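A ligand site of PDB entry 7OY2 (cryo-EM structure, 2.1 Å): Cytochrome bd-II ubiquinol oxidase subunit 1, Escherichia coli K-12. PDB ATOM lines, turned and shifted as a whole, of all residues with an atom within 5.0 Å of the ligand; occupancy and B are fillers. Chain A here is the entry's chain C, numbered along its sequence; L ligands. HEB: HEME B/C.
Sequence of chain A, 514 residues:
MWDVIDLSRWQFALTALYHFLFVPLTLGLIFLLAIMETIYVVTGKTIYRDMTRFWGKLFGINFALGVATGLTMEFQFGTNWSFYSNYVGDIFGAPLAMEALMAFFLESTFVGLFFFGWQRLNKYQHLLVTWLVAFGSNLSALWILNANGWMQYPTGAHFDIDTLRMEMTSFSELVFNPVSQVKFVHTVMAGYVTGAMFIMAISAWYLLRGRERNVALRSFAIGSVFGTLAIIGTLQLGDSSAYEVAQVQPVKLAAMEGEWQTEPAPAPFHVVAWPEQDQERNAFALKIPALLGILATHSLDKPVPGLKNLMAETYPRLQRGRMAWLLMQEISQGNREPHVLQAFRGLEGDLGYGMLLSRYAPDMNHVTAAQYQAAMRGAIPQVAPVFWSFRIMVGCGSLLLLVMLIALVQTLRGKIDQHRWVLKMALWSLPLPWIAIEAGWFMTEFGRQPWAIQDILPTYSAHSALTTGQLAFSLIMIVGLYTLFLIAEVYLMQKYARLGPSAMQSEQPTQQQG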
ATOM      1  N   PHE A  20      12.238  26.748  -5.320  1.00  0.00           N
ATOM      2  CA  PHE A  20      12.478  25.855  -6.435  1.00  0.00           C
ATOM      3  C   PHE A  20      12.729  26.606  -7.742  1.00  0.00           C
ATOM      4  O   PHE A  20      12.720  25.981  -8.805  1.00  0.00           O
ATOM      5  CB  PHE A  20      11.329  24.877  -6.618  1.00  0.00           C
ATOM      6  CG  PHE A  20      11.788  23.468  -6.919  1.00  0.00           C
ATOM      7  CD1 PHE A  20      12.365  22.687  -5.933  1.00  0.00           C
ATOM      8  CD2 PHE A  20      11.686  22.947  -8.184  1.00  0.00           C
ATOM      9  CE1 PHE A  20      12.791  21.401  -6.207  1.00  0.00           C
ATOM     10  CE2 PHE A  20      12.124  21.671  -8.464  1.00  0.00           C
ATOM     11  CZ  PHE A  20      12.672  20.896  -7.482  1.00  0.00           C
ATOM     12  N   LEU A 145      11.033  14.843  -0.813  1.00  0.00           N
ATOM     13  CA  LEU A 145      10.059  14.336  -1.761  1.00  0.00           C
ATOM     14  C   LEU A 145       9.373  13.092  -1.220  1.00  0.00           C
ATOM     15  O   LEU A 145       8.245  12.799  -1.623  1.00  0.00           O
ATOM     16  CB  LEU A 145      10.713  14.069  -3.104  1.00  0.00           C
ATOM     17  CG  LEU A 145      11.158  15.331  -3.848  1.00  0.00           C
ATOM     18  CD1 LEU A 145      11.948  14.994  -5.087  1.00  0.00           C
ATOM     19  CD2 LEU A 145       9.955  16.194  -4.182  1.00  0.00           C
ATOM     20  N   GLN A 152       0.844  13.039  -0.987  1.00  0.00           N
ATOM     21  CA  GLN A 152       0.048  12.601  -2.132  1.00  0.00           C
ATOM     22  C   GLN A 152      -0.571  11.237  -1.886  1.00  0.00           C
ATOM     23  O   GLN A 152      -1.710  10.980  -2.302  1.00  0.00           O
ATOM     24  CB  GLN A 152       0.896  12.571  -3.401  1.00  0.00           C
ATOM     25  CG  GLN A 152       1.862  13.738  -3.596  1.00  0.00           C
ATOM     26  CD  GLN A 152       1.167  15.077  -3.629  1.00  0.00           C
ATOM     27  OE1 GLN A 152      -0.025  15.175  -3.905  1.00  0.00           O
ATOM     28  NE2 GLN A 152       1.917  16.136  -3.370  1.00  0.00           N
ATOM     29  N   VAL A 179       4.866   6.365  -4.864  1.00  0.00           N
ATOM     30  CA  VAL A 179       4.759   7.751  -5.299  1.00  0.00           C
ATOM     31  C   VAL A 179       6.033   8.521  -4.967  1.00  0.00           C
ATOM     32  O   VAL A 179       6.571   9.240  -5.799  1.00  0.00           O
ATOM     33  CB  VAL A 179       3.530   8.414  -4.677  1.00  0.00           C
ATOM     34  CG1 VAL A 179       3.554   9.913  -4.916  1.00  0.00           C
ATOM     35  CG2 VAL A 179       2.271   7.815  -5.233  1.00  0.00           C
ATOM     36  N   LYS A 183       8.537  10.196  -7.631  1.00  0.00           N
ATOM     37  CA  LYS A 183       8.653  11.649  -7.472  1.00  0.00           C
ATOM     38  C   LYS A 183      10.107  12.057  -7.308  1.00  0.00           C
ATOM     39  O   LYS A 183      10.581  12.975  -7.972  1.00  0.00           O
ATOM     40  CB  LYS A 183       7.828  12.097  -6.274  1.00  0.00           C
ATOM     41  CG  LYS A 183       8.003  13.560  -5.898  1.00  0.00           C
ATOM     42  CD  LYS A 183       7.065  13.956  -4.759  1.00  0.00           C
ATOM     43  CE  LYS A 183       5.621  13.749  -5.141  1.00  0.00           C
ATOM     44  NZ  LYS A 183       5.168  14.791  -6.104  1.00  0.00           N
ATOM     45  N   HIS A 186      12.041  11.415 -10.739  1.00  0.00           N
ATOM     46  CA  HIS A 186      11.602  12.367 -11.755  1.00  0.00           C
ATOM     47  C   HIS A 186      12.109  13.771 -11.463  1.00  0.00           C
ATOM     48  O   HIS A 186      12.632  14.459 -12.360  1.00  0.00           O
ATOM     49  CB  HIS A 186      10.090  12.367 -11.819  1.00  0.00           C
ATOM     50  CG  HIS A 186       9.555  13.086 -13.004  1.00  0.00           C
ATOM     51  ND1 HIS A 186      10.194  13.079 -14.226  1.00  0.00           N
ATOM     52  CD2 HIS A 186       8.462  13.860 -13.158  1.00  0.00           C
ATOM     53  CE1 HIS A 186       9.515  13.811 -15.077  1.00  0.00           C
ATOM     54  NE2 HIS A 186       8.449  14.277 -14.465  1.00  0.00           N
ATOM     55  N   THR A 187      11.948  14.230 -10.228  1.00  0.00           N
ATOM     56  CA  THR A 187      12.348  15.591  -9.886  1.00  0.00           C
ATOM     57  C   THR A 187      13.854  15.772 -10.038  1.00  0.00           C
ATOM     58  O   THR A 187      14.312  16.788 -10.562  1.00  0.00           O
ATOM     59  CB  THR A 187      11.884  15.951  -8.478  1.00  0.00           C
ATOM     60  OG1 THR A 187      10.498  15.667  -8.350  1.00  0.00           O
ATOM     61  CG2 THR A 187      12.116  17.415  -8.196  1.00  0.00           C
ATOM     62  N   ALA A 190      14.719  16.055 -13.609  1.00  0.00           N
ATOM     63  CA  ALA A 190      14.391  17.401 -14.060  1.00  0.00           C
ATOM     64  C   ALA A 190      15.467  18.404 -13.653  1.00  0.00           C
ATOM     65  O   ALA A 190      15.812  19.308 -14.422  1.00  0.00           O
ATOM     66  CB  ALA A 190      13.028  17.818 -13.512  1.00  0.00           C
ATOM     67  N   VAL A 193      18.352  18.023 -16.008  1.00  0.00           N
ATOM     68  CA  VAL A 193      17.999  18.751 -17.226  1.00  0.00           C
ATOM     69  C   VAL A 193      18.245  20.247 -17.059  1.00  0.00           C
ATOM     70  O   VAL A 193      18.783  20.910 -17.949  1.00  0.00           O
ATOM     71  CB  VAL A 193      16.541  18.462 -17.612  1.00  0.00           C
ATOM     72  CG1 VAL A 193      16.144  19.291 -18.833  1.00  0.00           C
ATOM     73  CG2 VAL A 193      16.321  16.978 -17.865  1.00  0.00           C
ATOM     74  N   ILE A 231      17.116  14.196 -19.754  1.00  0.00           N
ATOM     75  CA  ILE A 231      15.775  14.448 -20.273  1.00  0.00           C
ATOM     76  C   ILE A 231      15.099  13.129 -20.640  1.00  0.00           C
ATOM     77  O   ILE A 231      13.891  12.976 -20.460  1.00  0.00           O
ATOM     78  CB  ILE A 231      15.810  15.432 -21.456  1.00  0.00           C
ATOM     79  CG1 ILE A 231      14.401  15.926 -21.807  1.00  0.00           C
ATOM     80  CG2 ILE A 231      16.457  14.809 -22.697  1.00  0.00           C
ATOM     81  CD1 ILE A 231      13.724  16.666 -20.698  1.00  0.00           C
ATOM     82  N   THR A 234      14.042  11.818 -17.382  1.00  0.00           N
ATOM     83  CA  THR A 234      12.946  12.664 -16.935  1.00  0.00           C
ATOM     84  C   THR A 234      11.649  12.233 -17.581  1.00  0.00           C
ATOM     85  O   THR A 234      10.636  12.071 -16.896  1.00  0.00           O
ATOM     86  CB  THR A 234      13.237  14.136 -17.263  1.00  0.00           C
ATOM     87  OG1 THR A 234      14.457  14.556 -16.658  1.00  0.00           O
ATOM     88  CG2 THR A 234      12.120  15.022 -16.768  1.00  0.00           C
ATOM     89  N   LEU A 235      11.643  12.041 -18.894  1.00  0.00           N
ATOM     90  CA  LEU A 235      10.427  11.624 -19.582  1.00  0.00           C
ATOM     91  C   LEU A 235       9.963  10.235 -19.109  1.00  0.00           C
ATOM     92  O   LEU A 235       8.767  10.013 -18.882  1.00  0.00           O
ATOM     93  CB  LEU A 235      10.636  11.644 -21.099  1.00  0.00           C
ATOM     94  CG  LEU A 235      11.077  12.957 -21.766  1.00  0.00           C
ATOM     95  CD1 LEU A 235      10.817  12.950 -23.273  1.00  0.00           C
ATOM     96  CD2 LEU A 235      10.448  14.181 -21.129  1.00  0.00           C
ATOM     97  N   GLY A 238       8.672  10.515 -15.727  1.00  0.00           N
ATOM     98  CA  GLY A 238       7.422  11.240 -15.791  1.00  0.00           C
ATOM     99  C   GLY A 238       6.276  10.318 -16.126  1.00  0.00           C
ATOM    100  O   GLY A 238       5.194  10.429 -15.551  1.00  0.00           O
ATOM    101  N   ASP A 239       6.500   9.391 -17.053  1.00  0.00           N
ATOM    102  CA  ASP A 239       5.491   8.369 -17.324  1.00  0.00           C
ATOM    103  C   ASP A 239       5.271   7.481 -16.101  1.00  0.00           C
ATOM    104  O   ASP A 239       4.137   7.102 -15.799  1.00  0.00           O
ATOM    105  CB  ASP A 239       5.895   7.550 -18.544  1.00  0.00           C
ATOM    106  CG  ASP A 239       6.021   8.405 -19.795  1.00  0.00           C
ATOM    107  OD1 ASP A 239       5.149   9.266 -20.017  1.00  0.00           O
ATOM    108  OD2 ASP A 239       6.995   8.216 -20.553  1.00  0.00           O
ATOM    109  N   SER A 241       5.656   8.454 -12.928  1.00  0.00           N
ATOM    110  CA  SER A 241       4.904   9.293 -12.009  1.00  0.00           C
ATOM    111  C   SER A 241       3.444   9.373 -12.431  1.00  0.00           C
ATOM    112  O   SER A 241       2.537   9.318 -11.590  1.00  0.00           O
ATOM    113  CB  SER A 241       5.500  10.701 -11.941  1.00  0.00           C
ATOM    114  OG  SER A 241       6.838  10.683 -11.463  1.00  0.00           O
ATOM    115  N   ALA A 242       3.197   9.514 -13.736  1.00  0.00           N
ATOM    116  CA  ALA A 242       1.845   9.534 -14.247  1.00  0.00           C
ATOM    117  C   ALA A 242       1.112   8.251 -13.908  1.00  0.00           C
ATOM    118  O   ALA A 242      -0.044   8.268 -13.479  1.00  0.00           O
ATOM    119  CB  ALA A 242       1.853   9.767 -15.758  1.00  0.00           C
ATOM    120  N   VAL A 245       0.381   8.266  -9.951  1.00  0.00           N
ATOM    121  CA  VAL A 245      -0.728   9.148  -9.583  1.00  0.00           C
ATOM    122  C   VAL A 245      -2.019   8.694 -10.222  1.00  0.00           C
ATOM    123  O   VAL A 245      -3.105   9.006  -9.720  1.00  0.00           O
ATOM    124  CB  VAL A 245      -0.413  10.621  -9.926  1.00  0.00           C
ATOM    125  CG1 VAL A 245       0.999  10.993  -9.485  1.00  0.00           C
ATOM    126  CG2 VAL A 245      -0.632  10.884 -11.403  1.00  0.00           C
ATOM    127  N   GLN A 249      -4.329   8.929  -7.205  1.00  0.00           N
ATOM    128  CA  GLN A 249      -4.939  10.257  -7.201  1.00  0.00           C
ATOM    129  C   GLN A 249      -5.843  10.431  -8.412  1.00  0.00           C
ATOM    130  O   GLN A 249      -5.378  10.871  -9.474  1.00  0.00           O
ATOM    131  CB  GLN A 249      -3.882  11.357  -7.142  1.00  0.00           C
ATOM    132  CG  GLN A 249      -3.604  11.844  -5.732  1.00  0.00           C
ATOM    133  CD  GLN A 249      -2.314  12.631  -5.605  1.00  0.00           C
ATOM    134  OE1 GLN A 249      -1.380  12.439  -6.371  1.00  0.00           O
ATOM    135  NE2 GLN A 249      -2.266  13.527  -4.618  1.00  0.00           N
ATOM    136  N   LYS A 252      -5.563  14.058 -10.404  1.00  0.00           N
ATOM    137  CA  LYS A 252      -4.455  14.248 -11.325  1.00  0.00           C
ATOM    138  C   LYS A 252      -4.547  13.277 -12.500  1.00  0.00           C
ATOM    139  O   LYS A 252      -4.069  13.589 -13.594  1.00  0.00           O
ATOM    140  CB  LYS A 252      -3.122  14.079 -10.593  1.00  0.00           C
ATOM    141  CG  LYS A 252      -2.888  15.146  -9.553  1.00  0.00           C
ATOM    142  CD  LYS A 252      -1.602  14.913  -8.796  1.00  0.00           C
ATOM    143  CE  LYS A 252      -1.480  15.861  -7.631  1.00  0.00           C
ATOM    144  NZ  LYS A 252      -0.446  15.425  -6.687  1.00  0.00           N
ATOM    145  N   MET A 256      -4.635  14.668 -16.729  1.00  0.00           N
ATOM    146  CA  MET A 256      -3.899  14.188 -17.923  1.00  0.00           C
ATOM    147  C   MET A 256      -4.864  13.553 -18.935  1.00  0.00           C
ATOM    148  O   MET A 256      -4.493  13.454 -20.123  1.00  0.00           O
ATOM    149  CB  MET A 256      -2.852  13.153 -17.511  1.00  0.00           C
ATOM    150  CG  MET A 256      -2.130  13.528 -16.230  1.00  0.00           C
ATOM    151  SD  MET A 256      -0.883  12.321 -15.717  1.00  0.00           S
ATOM    152  CE  MET A 256      -1.946  11.019 -15.071  1.00  0.00           C
ATOM    153  N   PHE A 390       0.135  20.385 -16.440  1.00  0.00           N
ATOM    154  CA  PHE A 390       0.640  19.112 -17.001  1.00  0.00           C
ATOM    155  C   PHE A 390       1.103  19.362 -18.443  1.00  0.00           C
ATOM    156  O   PHE A 390       2.178  18.953 -18.795  1.00  0.00           O
ATOM    157  CB  PHE A 390      -0.451  18.033 -17.082  1.00  0.00           C
ATOM    158  CG  PHE A 390       0.028  16.687 -17.563  1.00  0.00           C
ATOM    159  CD1 PHE A 390       0.981  15.982 -16.848  1.00  0.00           C
ATOM    160  CD2 PHE A 390      -0.458  16.128 -18.719  1.00  0.00           C
ATOM    161  CE1 PHE A 390       1.442  14.749 -17.280  1.00  0.00           C
ATOM    162  CE2 PHE A 390      -0.007  14.898 -19.152  1.00  0.00           C
ATOM    163  CZ  PHE A 390       0.938  14.214 -18.432  1.00  0.00           C
ATOM    164  N   MET A 393       4.338  21.316 -18.781  1.00  0.00           N
ATOM    165  CA  MET A 393       5.436  20.431 -18.328  1.00  0.00           C
ATOM    166  C   MET A 393       5.802  19.444 -19.432  1.00  0.00           C
ATOM    167  O   MET A 393       6.959  19.384 -19.787  1.00  0.00           O
ATOM    168  CB  MET A 393       5.064  19.749 -17.027  1.00  0.00           C
ATOM    169  CG  MET A 393       5.977  18.608 -16.662  1.00  0.00           C
ATOM    170  SD  MET A 393       5.409  17.715 -15.207  1.00  0.00           S
ATOM    171  CE  MET A 393       3.784  17.218 -15.738  1.00  0.00           C
ATOM    172  N   VAL A 394       4.809  18.750 -19.959  1.00  0.00           N
ATOM    173  CA  VAL A 394       5.069  17.701 -20.986  1.00  0.00           C
ATOM    174  C   VAL A 394       5.622  18.400 -22.244  1.00  0.00           C
ATOM    175  O   VAL A 394       6.719  17.965 -22.693  1.00  0.00           O
ATOM    176  CB  VAL A 394       3.848  16.799 -21.216  1.00  0.00           C
ATOM    177  CG1 VAL A 394       4.074  15.808 -22.350  1.00  0.00           C
ATOM    178  CG2 VAL A 394       3.483  16.064 -19.949  1.00  0.00           C
ATOM    179  N   GLY A 397       9.028  19.535 -21.924  1.00  0.00           N
ATOM    180  CA  GLY A 397       9.880  18.368 -21.971  1.00  0.00           C
ATOM    181  C   GLY A 397      10.181  17.902 -23.379  1.00  0.00           C
ATOM    182  O   GLY A 397      11.305  17.518 -23.693  1.00  0.00           O
ATOM    183  N   LEU A 400      12.626  20.286 -24.845  1.00  0.00           N
ATOM    184  CA  LEU A 400      13.936  20.037 -24.256  1.00  0.00           C
ATOM    185  C   LEU A 400      14.583  18.793 -24.833  1.00  0.00           C
ATOM    186  O   LEU A 400      15.785  18.760 -25.054  1.00  0.00           O
ATOM    187  CB  LEU A 400      13.824  19.929 -22.733  1.00  0.00           C
ATOM    188  CG  LEU A 400      13.724  21.259 -22.007  1.00  0.00           C
ATOM    189  CD1 LEU A 400      13.320  21.070 -20.547  1.00  0.00           C
ATOM    190  CD2 LEU A 400      15.036  22.010 -22.118  1.00  0.00           C
ATOM    191  N   PRO A 433      13.467  24.521 -18.795  1.00  0.00           N
ATOM    192  CA  PRO A 433      13.418  23.610 -17.637  1.00  0.00           C
ATOM    193  C   PRO A 433      12.683  24.209 -16.453  1.00  0.00           C
ATOM    194  O   PRO A 433      11.884  23.512 -15.829  1.00  0.00           O
ATOM    195  CB  PRO A 433      14.896  23.353 -17.334  1.00  0.00           C
ATOM    196  CG  PRO A 433      15.620  23.696 -18.569  1.00  0.00           C
ATOM    197  CD  PRO A 433      14.845  24.779 -19.217  1.00  0.00           C
ATOM    198  N   ALA A 436       8.869  24.106 -17.199  1.00  0.00           N
ATOM    199  CA  ALA A 436       8.326  22.762 -17.016  1.00  0.00           C
ATOM    200  C   ALA A 436       8.325  22.353 -15.552  1.00  0.00           C
ATOM    201  O   ALA A 436       7.411  21.668 -15.096  1.00  0.00           O
ATOM    202  CB  ALA A 436       9.116  21.755 -17.846  1.00  0.00           C
ATOM    203  N   ILE A 437       9.343  22.756 -14.803  1.00  0.00           N
ATOM    204  CA  ILE A 437       9.447  22.345 -13.413  1.00  0.00           C
ATOM    205  C   ILE A 437       8.370  23.018 -12.576  1.00  0.00           C
ATOM    206  O   ILE A 437       7.694  22.374 -11.763  1.00  0.00           O
ATOM    207  CB  ILE A 437      10.851  22.637 -12.879  1.00  0.00           C
ATOM    208  CG1 ILE A 437      11.811  21.567 -13.362  1.00  0.00           C
ATOM    209  CG2 ILE A 437      10.827  22.769 -11.387  1.00  0.00           C
ATOM    210  CD1 ILE A 437      13.212  21.926 -13.117  1.00  0.00           C
ATOM    211  N   GLY A 440       5.188  21.362 -13.320  1.00  0.00           N
ATOM    212  CA  GLY A 440       5.041  20.085 -12.654  1.00  0.00           C
ATOM    213  C   GLY A 440       4.708  20.243 -11.189  1.00  0.00           C
ATOM    214  O   GLY A 440       3.858  19.527 -10.654  1.00  0.00           O
ATOM    215  N   TRP A 441       5.327  21.211 -10.539  1.00  0.00           N
ATOM    216  CA  TRP A 441       5.051  21.418  -9.122  1.00  0.00           C
ATOM    217  C   TRP A 441       3.692  22.064  -8.913  1.00  0.00           C
ATOM    218  O   TRP A 441       2.994  21.750  -7.929  1.00  0.00           O
ATOM    219  CB  TRP A 441       6.162  22.235  -8.494  1.00  0.00           C
ATOM    220  CG  TRP A 441       7.218  21.387  -7.870  1.00  0.00           C
ATOM    221  CD1 TRP A 441       8.528  21.325  -8.215  1.00  0.00           C
ATOM    222  CD2 TRP A 441       7.035  20.456  -6.799  1.00  0.00           C
ATOM    223  NE1 TRP A 441       9.185  20.422  -7.414  1.00  0.00           N
ATOM    224  CE2 TRP A 441       8.289  19.872  -6.538  1.00  0.00           C
ATOM    225  CE3 TRP A 441       5.939  20.087  -6.020  1.00  0.00           C
ATOM    226  CZ2 TRP A 441       8.465  18.935  -5.530  1.00  0.00           C
ATOM    227  CZ3 TRP A 441       6.118  19.146  -5.035  1.00  0.00           C
ATOM    228  CH2 TRP A 441       7.377  18.576  -4.789  1.00  0.00           C
ATOM    229  N   MET A 443       1.099  21.455 -10.832  1.00  0.00           N
ATOM    230  CA  MET A 443       0.212  20.306 -10.975  1.00  0.00           C
ATOM    231  C   MET A 443       0.227  19.451  -9.714  1.00  0.00           C
ATOM    232  O   MET A 443      -0.829  19.053  -9.210  1.00  0.00           O
ATOM    233  CB  MET A 443       0.629  19.468 -12.175  1.00  0.00           C
ATOM    234  CG  MET A 443       0.025  18.073 -12.178  1.00  0.00           C
ATOM    235  SD  MET A 443       0.629  17.015 -13.495  1.00  0.00           S
ATOM    236  CE  MET A 443      -0.432  15.583 -13.255  1.00  0.00           C
ATOM    237  N   THR A 444       1.421  19.204  -9.224  1.00  0.00           N
ATOM    238  CA  THR A 444       1.583  18.393  -7.995  1.00  0.00           C
ATOM    239  C   THR A 444       0.830  19.004  -6.811  1.00  0.00           C
ATOM    240  O   THR A 444       0.048  18.261  -6.217  1.00  0.00           O
ATOM    241  CB  THR A 444       3.051  18.106  -7.659  1.00  0.00           C
ATOM    242  OG1 THR A 444       3.581  17.329  -8.724  1.00  0.00           O
ATOM    243  CG2 THR A 444       3.218  17.428  -6.318  1.00  0.00           C
HETATM  244 FE   HEB L   1       6.898  15.980 -14.788  1.00  0.00          FE
HETATM  245  CHA HEB L   1       5.570  16.217 -11.352  1.00  0.00           C
HETATM  246  CHB HEB L   1       4.362  13.463 -15.633  1.00  0.00           C
HETATM  247  CHC HEB L   1       8.264  15.783 -18.164  1.00  0.00           C
HETATM  248  CHD HEB L   1       9.586  18.549 -14.004  1.00  0.00           C
HETATM  249  NA  HEB L   1       5.345  15.065 -13.684  1.00  0.00           N
HETATM  250  C1A HEB L   1       4.973  15.321 -12.316  1.00  0.00           C
HETATM  251  C2A HEB L   1       3.975  14.495 -12.193  1.00  0.00           C
HETATM  252  C3A HEB L   1       3.599  13.810 -13.148  1.00  0.00           C
HETATM  253  C4A HEB L   1       4.371  14.016 -14.262  1.00  0.00           C
HETATM  254  CMA HEB L   1       2.433  12.838 -13.099  1.00  0.00           C
HETATM  255  CAA HEB L   1       3.212  14.421 -10.860  1.00  0.00           C
HETATM  256  CBA HEB L   1       3.952  13.789  -9.704  1.00  0.00           C
HETATM  257  CGA HEB L   1       3.068  13.985  -8.481  1.00  0.00           C
HETATM  258  O1A HEB L   1       3.479  13.624  -7.351  1.00  0.00           O
HETATM  259  O2A HEB L   1       1.926  14.505  -8.610  1.00  0.00           O
HETATM  260  NB  HEB L   1       6.417  14.836 -16.548  1.00  0.00           N
HETATM  261  C1B HEB L   1       5.322  13.866 -16.675  1.00  0.00           C
HETATM  262  C2B HEB L   1       5.492  13.521 -17.908  1.00  0.00           C
HETATM  263  C3B HEB L   1       6.411  14.022 -18.593  1.00  0.00           C
HETATM  264  C4B HEB L   1       7.119  14.931 -17.856  1.00  0.00           C
HETATM  265  CMB HEB L   1       4.523  12.489 -18.438  1.00  0.00           C
HETATM  266  CAB HEB L   1       6.745  13.758 -20.056  1.00  0.00           C
HETATM  267  CBB HEB L   1       7.175  12.359 -20.413  1.00  0.00           C
HETATM  268  NC  HEB L   1       8.555  16.984 -15.741  1.00  0.00           N
HETATM  269  C1C HEB L   1       8.919  16.731 -17.183  1.00  0.00           C
HETATM  270  C2C HEB L   1       9.867  17.478 -17.339  1.00  0.00           C
HETATM  271  C3C HEB L   1      10.282  18.178 -16.414  1.00  0.00           C
HETATM  272  C4C HEB L   1       9.492  17.986 -15.236  1.00  0.00           C
HETATM  273  CMC HEB L   1      10.513  17.485 -18.715  1.00  0.00           C
HETATM  274  CAC HEB L   1      11.414  19.173 -16.421  1.00  0.00           C
HETATM  275  CBC HEB L   1      12.795  18.677 -16.786  1.00  0.00           C
HETATM  276  ND  HEB L   1       7.563  17.255 -12.944  1.00  0.00           N
HETATM  277  C1D HEB L   1       8.646  18.189 -12.904  1.00  0.00           C
HETATM  278  C2D HEB L   1       8.482  18.553 -11.632  1.00  0.00           C
HETATM  279  C3D HEB L   1       7.503  18.054 -10.822  1.00  0.00           C
HETATM  280  C4D HEB L   1       6.784  17.112 -11.655  1.00  0.00           C
HETATM  281  CMD HEB L   1       9.413  19.571 -11.072  1.00  0.00           C
HETATM  282  CAD HEB L   1       7.196  18.358  -9.363  1.00  0.00           C
HETATM  283  CBD HEB L   1       7.882  17.286  -8.540  1.00  0.00           C
HETATM  284  CGD HEB L   1       7.087  15.990  -8.651  1.00  0.00           C
HETATM  285  O1D HEB L   1       7.583  14.997  -9.232  1.00  0.00           O
HETATM  286  O2D HEB L   1       5.928  15.912  -8.186  1.00  0.00           O
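N of Gly 238 lies within hydrogen-bond range of ND1 of His 186 (3.3 Å).
The backbone carbonyl oxygen of Thr 234 sits close to a ring nitrogen (ND1) of His 186, at 2.9 Å.
The backbone carbonyl oxygen (O) of Lys 183 sits at hydrogen-bond distance from the side-chain hydroxyl (OG1) of Thr 187.
O of Thr 444 lies within hydrogen-bond range of NZ of Lys 252 (2.9 Å).
The backbone carbonyl oxygen (O) of Gly 440 is in hydrogen-bond range of the side-chain hydroxyl (OG1) of Thr 444.
NZ of Lys 252 lies within hydrogen-bond range of OE1 of Gln 152, at 2.8 Å.
The side-chain amino group of Lys 252 sits at hydrogen-bond distance from the side-chain amide oxygen of Gln 249.
OG1 of Thr 234 lies within hydrogen-bond range of N of Ala 190 (3.4 Å).
Merely in contact with the ligand: Ala 190 (3.4 Å), Val 193 (3.8 Å), Ile 231 (3.9 Å), Thr 234 (3.4 Å), Leu 235 (3.2 Å), Gly 238 (3.1 Å), Asp 239 (3.6 Å), Ser 241 (3.7 Å), Ala 242 (3.5 Å), Val 245 (3.7 Å), Phe 390 (3.6 Å), Val 394 (3.8 Å), Gly 397 (3.4 Å), Ala 436 (3.7 Å), Ile 437 (3.4 Å), Gly 440 (3.6 Å), Trp 441 (3.3 Å) and Met 443 (3.97 Å).
Hydrophobic or aromatic side chains that line the ligand: His 186, Ala 190, Val 193, Ile 231, Leu 235, Val 245, Phe 390, Met 393, Val 394, Ala 436, Ile 437, Trp 441 and Met 443.
24 residues have an atom within 4 Å of the ligand: Lys 183, His 186, Thr 187, Ala 190, Val 193, Ile 231, Thr 234, Leu 235, Gly 238, Asp 239, Ser 241, Ala 242, Val 245, Lys 252, Phe 390, Met 393, Val 394, Gly 397, Ala 436, Ile 437, Gly 440, Trp 441, Met 443 and Thr 444.
SD of Met 393 is bound to FE of the ligand (2.3 Å).
An iron atom (FE) of the ligand is bound by a ring nitrogen (NE2) of His 186, 2.3 Å away.
The side-chain amino group (NZ) of Lys 183 lies within salt-bridge range of an oxygen (O1A) of the ligand (2.4 Å).
The side-chain hydroxyl of Thr 444 sits at hydrogen-bond distance from an oxygen (O2D) of the ligand.
OG1 of Thr 187 lies close to O1D of the ligand, at 3.1 Å.
NZ of Lys 252 is in salt-bridge range of O2A of the ligand, at 3.2 Å.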
